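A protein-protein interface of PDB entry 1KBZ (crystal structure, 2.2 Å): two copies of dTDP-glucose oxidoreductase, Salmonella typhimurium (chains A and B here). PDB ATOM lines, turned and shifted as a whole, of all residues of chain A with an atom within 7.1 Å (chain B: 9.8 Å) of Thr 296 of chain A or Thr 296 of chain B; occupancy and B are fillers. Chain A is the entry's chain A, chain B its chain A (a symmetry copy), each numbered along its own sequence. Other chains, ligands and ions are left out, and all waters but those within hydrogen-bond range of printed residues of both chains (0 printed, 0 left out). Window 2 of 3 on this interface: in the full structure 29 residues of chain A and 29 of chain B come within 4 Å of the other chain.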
ATOM      1  N   LYS A 164     -23.423 -19.618   2.462  1.00  0.00           N
ATOM      2  CA  LYS A 164     -24.727 -19.027   2.221  1.00  0.00           C
ATOM      3  C   LYS A 164     -25.861 -19.888   2.783  1.00  0.00           C
ATOM      4  O   LYS A 164     -26.659 -19.430   3.614  1.00  0.00           O
ATOM      5  CB  LYS A 164     -24.931 -18.799   0.728  1.00  0.00           C
ATOM      6  CG  LYS A 164     -24.256 -17.535   0.205  1.00  0.00           C
ATOM      7  CD  LYS A 164     -24.657 -17.220  -1.242  1.00  0.00           C
ATOM      8  CE  LYS A 164     -23.723 -16.162  -1.845  1.00  0.00           C
ATOM      9  NZ  LYS A 164     -23.887 -16.009  -3.317  1.00  0.00           N
ATOM     10  N   THR A 291     -16.672 -11.382   3.339  1.00  0.00           N
ATOM     11  CA  THR A 291     -16.624  -9.925   3.287  1.00  0.00           C
ATOM     12  C   THR A 291     -17.295  -9.379   2.021  1.00  0.00           C
ATOM     13  O   THR A 291     -17.998  -8.377   2.077  1.00  0.00           O
ATOM     14  CB  THR A 291     -15.198  -9.435   3.357  1.00  0.00           C
ATOM     15  OG1 THR A 291     -14.603  -9.889   4.578  1.00  0.00           O
ATOM     16  CG2 THR A 291     -15.154  -7.945   3.464  1.00  0.00           C
ATOM     17  N   GLU A 292     -17.087 -10.055   0.896  1.00  0.00           N
ATOM     18  CA  GLU A 292     -17.667  -9.619  -0.372  1.00  0.00           C
ATOM     19  C   GLU A 292     -19.186  -9.799  -0.285  1.00  0.00           C
ATOM     20  O   GLU A 292     -19.936  -8.912  -0.640  1.00  0.00           O
ATOM     21  CB  GLU A 292     -17.072 -10.363  -1.589  1.00  0.00           C
ATOM     22  CG  GLU A 292     -15.691  -9.843  -2.006  1.00  0.00           C
ATOM     23  CD  GLU A 292     -15.176 -10.465  -3.312  1.00  0.00           C
ATOM     24  OE1 GLU A 292     -15.676 -11.546  -3.682  1.00  0.00           O
ATOM     25  OE2 GLU A 292     -14.321  -9.861  -3.983  1.00  0.00           O
ATOM     26  N   MET A 293     -19.621 -10.943   0.183  1.00  0.00           N
ATOM     27  CA  MET A 293     -21.029 -11.159   0.404  1.00  0.00           C
ATOM     28  C   MET A 293     -21.643 -10.093   1.362  1.00  0.00           C
ATOM     29  O   MET A 293     -22.680  -9.522   1.054  1.00  0.00           O
ATOM     30  CB  MET A 293     -21.241 -12.532   1.016  1.00  0.00           C
ATOM     31  CG  MET A 293     -21.100 -13.713   0.084  1.00  0.00           C
ATOM     32  SD  MET A 293     -21.542 -15.238   1.026  1.00  0.00           S
ATOM     33  CE  MET A 293     -23.041 -14.693   1.796  1.00  0.00           C
ATOM     34  N   PHE A 294     -21.009  -9.816   2.497  1.00  0.00           N
ATOM     35  CA  PHE A 294     -21.542  -8.829   3.456  1.00  0.00           C
ATOM     36  C   PHE A 294     -21.353  -7.372   3.052  1.00  0.00           C
ATOM     37  O   PHE A 294     -21.940  -6.501   3.659  1.00  0.00           O
ATOM     38  CB  PHE A 294     -20.905  -8.997   4.838  1.00  0.00           C
ATOM     39  CG  PHE A 294     -20.999 -10.375   5.386  1.00  0.00           C
ATOM     40  CD1 PHE A 294     -22.037 -11.209   5.041  1.00  0.00           C
ATOM     41  CD2 PHE A 294     -20.043 -10.834   6.248  1.00  0.00           C
ATOM     42  CE1 PHE A 294     -22.123 -12.463   5.564  1.00  0.00           C
ATOM     43  CE2 PHE A 294     -20.130 -12.092   6.787  1.00  0.00           C
ATOM     44  CZ  PHE A 294     -21.169 -12.907   6.449  1.00  0.00           C
ATOM     45  N   THR A 295     -20.524  -7.076   2.056  1.00  0.00           N
ATOM     46  CA  THR A 295     -20.344  -5.672   1.685  1.00  0.00           C
ATOM     47  C   THR A 295     -20.976  -5.412   0.344  1.00  0.00           C
ATOM     48  O   THR A 295     -20.310  -5.020  -0.605  1.00  0.00           O
ATOM     49  CB  THR A 295     -18.873  -5.196   1.721  1.00  0.00           C
ATOM     50  OG1 THR A 295     -18.084  -5.877   0.731  1.00  0.00           O
ATOM     51  CG2 THR A 295     -18.224  -5.526   3.089  1.00  0.00           C
ATOM     52  N   THR A 296     -22.280  -5.656   0.292  1.00  0.00           N
ATOM     53  CA  THR A 296     -23.081  -5.358  -0.883  1.00  0.00           C
ATOM     54  C   THR A 296     -23.902  -4.096  -0.640  1.00  0.00           C
ATOM     55  O   THR A 296     -24.577  -3.968   0.392  1.00  0.00           O
ATOM     56  CB  THR A 296     -24.044  -6.526  -1.215  1.00  0.00           C
ATOM     57  OG1 THR A 296     -23.301  -7.678  -1.660  1.00  0.00           O
ATOM     58  CG2 THR A 296     -24.915  -6.172  -2.408  1.00  0.00           C
ATOM     59  N   THR A 297     -23.826  -3.170  -1.596  1.00  0.00           N
ATOM     60  CA  THR A 297     -24.635  -1.949  -1.594  1.00  0.00           C
ATOM     61  C   THR A 297     -25.303  -1.871  -2.974  1.00  0.00           C
ATOM     62  O   THR A 297     -25.014  -2.693  -3.851  1.00  0.00           O
ATOM     63  CB  THR A 297     -23.733  -0.689  -1.371  1.00  0.00           C
ATOM     64  OG1 THR A 297     -22.922  -0.856  -0.201  1.00  0.00           O
ATOM     65  CG2 THR A 297     -24.548   0.576  -1.069  1.00  0.00           C
ATOM     66  N   THR A 298     -26.208  -0.912  -3.159  1.00  0.00           N
ATOM     67  CA  THR A 298     -26.797  -0.659  -4.474  1.00  0.00           C
ATOM     68  C   THR A 298     -27.247   0.796  -4.556  1.00  0.00           C
ATOM     69  O   THR A 298     -27.076   1.560  -3.603  1.00  0.00           O
ATOM     70  CB  THR A 298     -27.986  -1.599  -4.754  1.00  0.00           C
ATOM     71  OG1 THR A 298     -27.583  -2.968  -4.576  1.00  0.00           O
ATOM     72  CG2 THR A 298     -28.408  -1.519  -6.231  1.00  0.00           C
ATOM     73  N   GLY B 157     -15.708  -3.842  -8.861  1.00  0.00           N
ATOM     74  CA  GLY B 157     -17.066  -4.122  -8.417  1.00  0.00           C
ATOM     75  C   GLY B 157     -17.198  -3.995  -6.903  1.00  0.00           C
ATOM     76  O   GLY B 157     -18.291  -3.992  -6.386  1.00  0.00           O
ATOM     77  N   LYS B 158     -16.094  -3.886  -6.183  1.00  0.00           N
ATOM     78  CA  LYS B 158     -16.176  -3.704  -4.755  1.00  0.00           C
ATOM     79  C   LYS B 158     -16.036  -2.209  -4.490  1.00  0.00           C
ATOM     80  O   LYS B 158     -15.012  -1.580  -4.811  1.00  0.00           O
ATOM     81  CB  LYS B 158     -15.094  -4.483  -4.003  1.00  0.00           C
ATOM     82  CG  LYS B 158     -15.264  -4.406  -2.481  1.00  0.00           C
ATOM     83  CD  LYS B 158     -14.206  -5.181  -1.761  1.00  0.00           C
ATOM     84  CE  LYS B 158     -14.143  -4.860  -0.288  1.00  0.00           C
ATOM     85  NZ  LYS B 158     -15.139  -5.672   0.425  1.00  0.00           N
ATOM     86  N   GLY B 159     -17.078  -1.637  -3.935  1.00  0.00           N
ATOM     87  CA  GLY B 159     -17.062  -0.229  -3.658  1.00  0.00           C
ATOM     88  C   GLY B 159     -17.552   0.579  -4.845  1.00  0.00           C
ATOM     89  O   GLY B 159     -18.065   0.053  -5.846  1.00  0.00           O
ATOM     90  N   ASN B 160     -17.357   1.882  -4.730  1.00  0.00           N
ATOM     91  CA  ASN B 160     -17.843   2.822  -5.723  1.00  0.00           C
ATOM     92  C   ASN B 160     -17.115   2.770  -7.065  1.00  0.00           C
ATOM     93  O   ASN B 160     -15.905   2.548  -7.112  1.00  0.00           O
ATOM     94  CB  ASN B 160     -17.748   4.230  -5.155  1.00  0.00           C
ATOM     95  CG  ASN B 160     -18.504   5.208  -5.982  1.00  0.00           C
ATOM     96  OD1 ASN B 160     -19.736   5.267  -5.907  1.00  0.00           O
ATOM     97  ND2 ASN B 160     -17.785   5.969  -6.814  1.00  0.00           N
ATOM     98  N   LYS B 164     -21.614   2.335 -11.161  1.00  0.00           N
ATOM     99  CA  LYS B 164     -22.511   2.480 -10.028  1.00  0.00           C
ATOM    100  C   LYS B 164     -23.061   3.902  -9.908  1.00  0.00           C
ATOM    101  O   LYS B 164     -24.282   4.118  -9.921  1.00  0.00           O
ATOM    102  CB  LYS B 164     -21.798   2.081  -8.742  1.00  0.00           C
ATOM    103  CG  LYS B 164     -21.743   0.574  -8.514  1.00  0.00           C
ATOM    104  CD  LYS B 164     -21.217   0.217  -7.117  1.00  0.00           C
ATOM    105  CE  LYS B 164     -20.857  -1.273  -7.040  1.00  0.00           C
ATOM    106  NZ  LYS B 164     -20.095  -1.626  -5.810  1.00  0.00           N
ATOM    107  N   ARG B 168     -26.945   4.955 -10.239  1.00  0.00           N
ATOM    108  CA  ARG B 168     -27.707   5.647  -9.197  1.00  0.00           C
ATOM    109  C   ARG B 168     -28.462   6.829  -9.788  1.00  0.00           C
ATOM    110  O   ARG B 168     -29.587   7.108  -9.391  1.00  0.00           O
ATOM    111  CB  ARG B 168     -26.798   6.143  -8.068  1.00  0.00           C
ATOM    112  CG  ARG B 168     -26.791   5.234  -6.860  1.00  0.00           C
ATOM    113  CD  ARG B 168     -26.067   5.790  -5.650  1.00  0.00           C
ATOM    114  NE  ARG B 168     -25.425   4.707  -4.906  1.00  0.00           N
ATOM    115  CZ  ARG B 168     -24.184   4.284  -5.121  1.00  0.00           C
ATOM    116  NH1 ARG B 168     -23.434   4.870  -6.044  1.00  0.00           N
ATOM    117  NH2 ARG B 168     -23.683   3.282  -4.405  1.00  0.00           N
ATOM    118  N   ALA B 237     -30.723  -6.592 -17.957  1.00  0.00           N
ATOM    119  CA  ALA B 237     -30.802  -7.363 -16.713  1.00  0.00           C
ATOM    120  C   ALA B 237     -32.130  -7.168 -15.962  1.00  0.00           C
ATOM    121  O   ALA B 237     -32.342  -7.731 -14.890  1.00  0.00           O
ATOM    122  CB  ALA B 237     -29.601  -7.015 -15.798  1.00  0.00           C
ATOM    123  N   ILE B 239     -33.202  -4.232 -14.840  1.00  0.00           N
ATOM    124  CA  ILE B 239     -33.162  -3.052 -13.988  1.00  0.00           C
ATOM    125  C   ILE B 239     -33.932  -1.950 -14.727  1.00  0.00           C
ATOM    126  O   ILE B 239     -33.548  -1.553 -15.832  1.00  0.00           O
ATOM    127  CB  ILE B 239     -31.733  -2.537 -13.720  1.00  0.00           C
ATOM    128  CG1 ILE B 239     -30.774  -3.647 -13.235  1.00  0.00           C
ATOM    129  CG2 ILE B 239     -31.789  -1.376 -12.731  1.00  0.00           C
ATOM    130  CD1 ILE B 239     -31.209  -4.353 -11.971  1.00  0.00           C
ATOM    131  N   MET B 289     -18.270  -7.218 -14.455  1.00  0.00           N
ATOM    132  CA  MET B 289     -18.484  -6.548 -13.170  1.00  0.00           C
ATOM    133  C   MET B 289     -20.006  -6.122 -13.006  1.00  0.00           C
ATOM    134  O   MET B 289     -20.560  -6.261 -11.931  1.00  0.00           O
ATOM    135  CB  MET B 289     -17.477  -5.445 -12.931  1.00  0.00           C
ATOM    136  CG  MET B 289     -17.840  -4.115 -13.384  1.00  0.00           C
ATOM    137  SD  MET B 289     -18.252  -3.005 -12.020  1.00  0.00           S
ATOM    138  CE  MET B 289     -18.295  -1.488 -12.937  1.00  0.00           C
ATOM    139  N   LEU B 290     -20.658  -5.688 -14.080  1.00  0.00           N
ATOM    140  CA  LEU B 290     -22.110  -5.405 -14.064  1.00  0.00           C
ATOM    141  C   LEU B 290     -22.971  -6.674 -13.738  1.00  0.00           C
ATOM    142  O   LEU B 290     -23.897  -6.617 -12.914  1.00  0.00           O
ATOM    143  CB  LEU B 290     -22.555  -4.742 -15.386  1.00  0.00           C
ATOM    144  CG  LEU B 290     -21.920  -3.354 -15.616  1.00  0.00           C
ATOM    145  CD1 LEU B 290     -22.212  -2.800 -16.982  1.00  0.00           C
ATOM    146  CD2 LEU B 290     -22.374  -2.357 -14.552  1.00  0.00           C
ATOM    147  N   THR B 291     -22.648  -7.809 -14.355  1.00  0.00           N
ATOM    148  CA  THR B 291     -23.350  -9.047 -14.037  1.00  0.00           C
ATOM    149  C   THR B 291     -23.213  -9.416 -12.555  1.00  0.00           C
ATOM    150  O   THR B 291     -24.172  -9.863 -11.938  1.00  0.00           O
ATOM    151  CB  THR B 291     -22.841 -10.184 -14.891  1.00  0.00           C
ATOM    152  OG1 THR B 291     -23.041  -9.861 -16.272  1.00  0.00           O
ATOM    153  CG2 THR B 291     -23.664 -11.414 -14.683  1.00  0.00           C
ATOM    154  N   GLU B 292     -22.027  -9.205 -11.995  1.00  0.00           N
ATOM    155  CA  GLU B 292     -21.778  -9.530 -10.593  1.00  0.00           C
ATOM    156  C   GLU B 292     -22.602  -8.569  -9.730  1.00  0.00           C
ATOM    157  O   GLU B 292     -23.267  -8.983  -8.803  1.00  0.00           O
ATOM    158  CB  GLU B 292     -20.278  -9.485 -10.224  1.00  0.00           C
ATOM    159  CG  GLU B 292     -19.501 -10.726 -10.682  1.00  0.00           C
ATOM    160  CD  GLU B 292     -18.053 -10.760 -10.170  1.00  0.00           C
ATOM    161  OE1 GLU B 292     -17.536  -9.684  -9.808  1.00  0.00           O
ATOM    162  OE2 GLU B 292     -17.458 -11.847 -10.088  1.00  0.00           O
ATOM    163  N   MET B 293     -22.548  -7.297 -10.045  1.00  0.00           N
ATOM    164  CA  MET B 293     -23.374  -6.335  -9.360  1.00  0.00           C
ATOM    165  C   MET B 293     -24.890  -6.691  -9.455  1.00  0.00           C
ATOM    166  O   MET B 293     -25.582  -6.684  -8.447  1.00  0.00           O
ATOM    167  CB  MET B 293     -23.165  -4.961  -9.970  1.00  0.00           C
ATOM    168  CG  MET B 293     -21.874  -4.258  -9.619  1.00  0.00           C
ATOM    169  SD  MET B 293     -21.926  -2.568 -10.361  1.00  0.00           S
ATOM    170  CE  MET B 293     -23.551  -2.070  -9.865  1.00  0.00           C
ATOM    171  N   PHE B 294     -25.396  -7.011 -10.643  1.00  0.00           N
ATOM    172  CA  PHE B 294     -26.824  -7.342 -10.807  1.00  0.00           C
ATOM    173  C   PHE B 294     -27.223  -8.730 -10.318  1.00  0.00           C
ATOM    174  O   PHE B 294     -28.397  -9.013 -10.211  1.00  0.00           O
ATOM    175  CB  PHE B 294     -27.252  -7.244 -12.273  1.00  0.00           C
ATOM    176  CG  PHE B 294     -26.932  -5.941 -12.913  1.00  0.00           C
ATOM    177  CD1 PHE B 294     -26.866  -4.783 -12.174  1.00  0.00           C
ATOM    178  CD2 PHE B 294     -26.697  -5.880 -14.257  1.00  0.00           C
ATOM    179  CE1 PHE B 294     -26.591  -3.592 -12.774  1.00  0.00           C
ATOM    180  CE2 PHE B 294     -26.430  -4.682 -14.869  1.00  0.00           C
ATOM    181  CZ  PHE B 294     -26.379  -3.538 -14.130  1.00  0.00           C
ATOM    182  N   THR B 295     -26.274  -9.619 -10.042  1.00  0.00           N
ATOM    183  CA  THR B 295     -26.671 -10.951  -9.582  1.00  0.00           C
ATOM    184  C   THR B 295     -26.314 -11.118  -8.131  1.00  0.00           C
ATOM    185  O   THR B 295     -25.538 -11.992  -7.765  1.00  0.00           O
ATOM    186  CB  THR B 295     -26.108 -12.106 -10.443  1.00  0.00           C
ATOM    187  OG1 THR B 295     -24.674 -12.166 -10.354  1.00  0.00           O
ATOM    188  CG2 THR B 295     -26.436 -11.883 -11.941  1.00  0.00           C
ATOM    189  N   THR B 296     -26.894 -10.245  -7.315  1.00  0.00           N
ATOM    190  CA  THR B 296     -26.759 -10.322  -5.870  1.00  0.00           C
ATOM    191  C   THR B 296     -28.039 -10.882  -5.261  1.00  0.00           C
ATOM    192  O   THR B 296     -29.146 -10.415  -5.572  1.00  0.00           O
ATOM    193  CB  THR B 296     -26.483  -8.925  -5.260  1.00  0.00           C
ATOM    194  OG1 THR B 296     -25.175  -8.457  -5.646  1.00  0.00           O
ATOM    195  CG2 THR B 296     -26.405  -9.013  -3.746  1.00  0.00           C
ATOM    196  N   THR B 297     -27.874 -11.889  -4.404  1.00  0.00           N
ATOM    197  CA  THR B 297     -28.973 -12.473  -3.632  1.00  0.00           C
ATOM    198  C   THR B 297     -28.517 -12.480  -2.167  1.00  0.00           C
ATOM    199  O   THR B 297     -27.365 -12.138  -1.873  1.00  0.00           O
ATOM    200  CB  THR B 297     -29.262 -13.937  -4.104  1.00  0.00           C
ATOM    201  OG1 THR B 297     -29.457 -13.976  -5.524  1.00  0.00           O
ATOM    202  CG2 THR B 297     -30.579 -14.491  -3.542  1.00  0.00           C
ATOM    203  N   THR B 298     -29.416 -12.837  -1.252  1.00  0.00           N
ATOM    204  CA  THR B 298     -29.048 -13.016   0.153  1.00  0.00           C
ATOM    205  C   THR B 298     -30.012 -13.999   0.809  1.00  0.00           C
ATOM    206  O   THR B 298     -30.920 -14.517   0.154  1.00  0.00           O
ATOM    207  CB  THR B 298     -29.052 -11.677   0.917  1.00  0.00           C
ATOM    208  OG1 THR B 298     -28.220 -10.721   0.239  1.00  0.00           O
ATOM    209  CG2 THR B 298     -28.396 -11.836   2.299  1.00  0.00           C
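The side-chain hydroxyl (OG1) of Thr 295 of chain A lies within hydrogen-bond range of the side-chain amino group (NZ) of Lys 158 of chain B (3.0 Å).
The backbone carbonyl oxygen (O) of Thr 291 of chain A lies within hydrogen-bond range of the side-chain hydroxyl (OG1) of Thr 295 of chain A (2.8 Å).
The backbone carbonyl oxygen of Met 293 of chain A is in hydrogen-bond range of the side-chain hydroxyl of Thr 296 of chain A, at 3.3 Å.
The backbone carbonyl oxygen of Met 293 of chain B is in hydrogen-bond range of the side-chain hydroxyl of Thr 296 of chain B (3.3 Å).
Among the printed residues, merely in contact across the chains: Thr 291 of chain A with Lys 158 of chain B (3.8 Å), Thr 296 of chain A with Thr 296 of chain B (3.5 Å) and Thr 298 of chain A with Arg 168 of chain B (3.8 Å).
Of the printed residues of chain B, Thr 291 of chain A touches Lys 158.
Thr 295 of chain A touches just one residue of chain B: Lys 158 (3.0 Å).
Of chain B, only Thr 296 comes within 4 Å of Thr 296 of chain A.
No residue of chain B comes within 4 Å of Thr 297 of chain A.
Printed residues of chain B within 4 Å of Thr 298 of chain A: Arg 168 (3.8 Å).
Of the printed residues of chain A, Lys 158 of chain B touches Thr 291 (3.8 Å) and Thr 295 (3.0 Å).
Printed residues of chain A within 4 Å of Arg 168 of chain B: Thr 298 (3.8 Å).
Glu 292 of chain B touches none of the printed residues of chain A.
Phe 294 of chain B touches none of the printed residues of chain A.
Thr 296 of chain B touches just one residue of chain A: Thr 296 (3.5 Å).
The nearest residue of chain A that does not touch Thr 296 of chain B is Thr 297 of chain A (6.0 Å).
The nearest printed residue of chain A that does not touch Lys 158 of chain B is Glu 292 of chain A (4.8 Å).
Of the 9 printed residues of chain A, 4 touch a printed residue of chain B.
Printed residues of chain A that touch a printed residue of chain B: Thr 291, Thr 295, Thr 296 and Thr 298.
Along chain A the printed residues that touch a printed residue of chain B span positions 291 to 298.
Printed residues of chain B that touch a printed residue of chain A: Lys 158, Arg 168 and Thr 296.
Among the printed residues, 4 pairs touch across the chains.
Among the printed residues, no Asp or Glu carboxylate lies within 4 Å of a Lys or Arg side-chain nitrogen of the other chain.
Thr 296 of chain B touches its own counterpart, Thr 296 of chain A.
9 positions are printed for both chains.
Of the 4 pairs that touch across the chains among the printed residues, 1 has its exchanged pair printed and touching as well.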
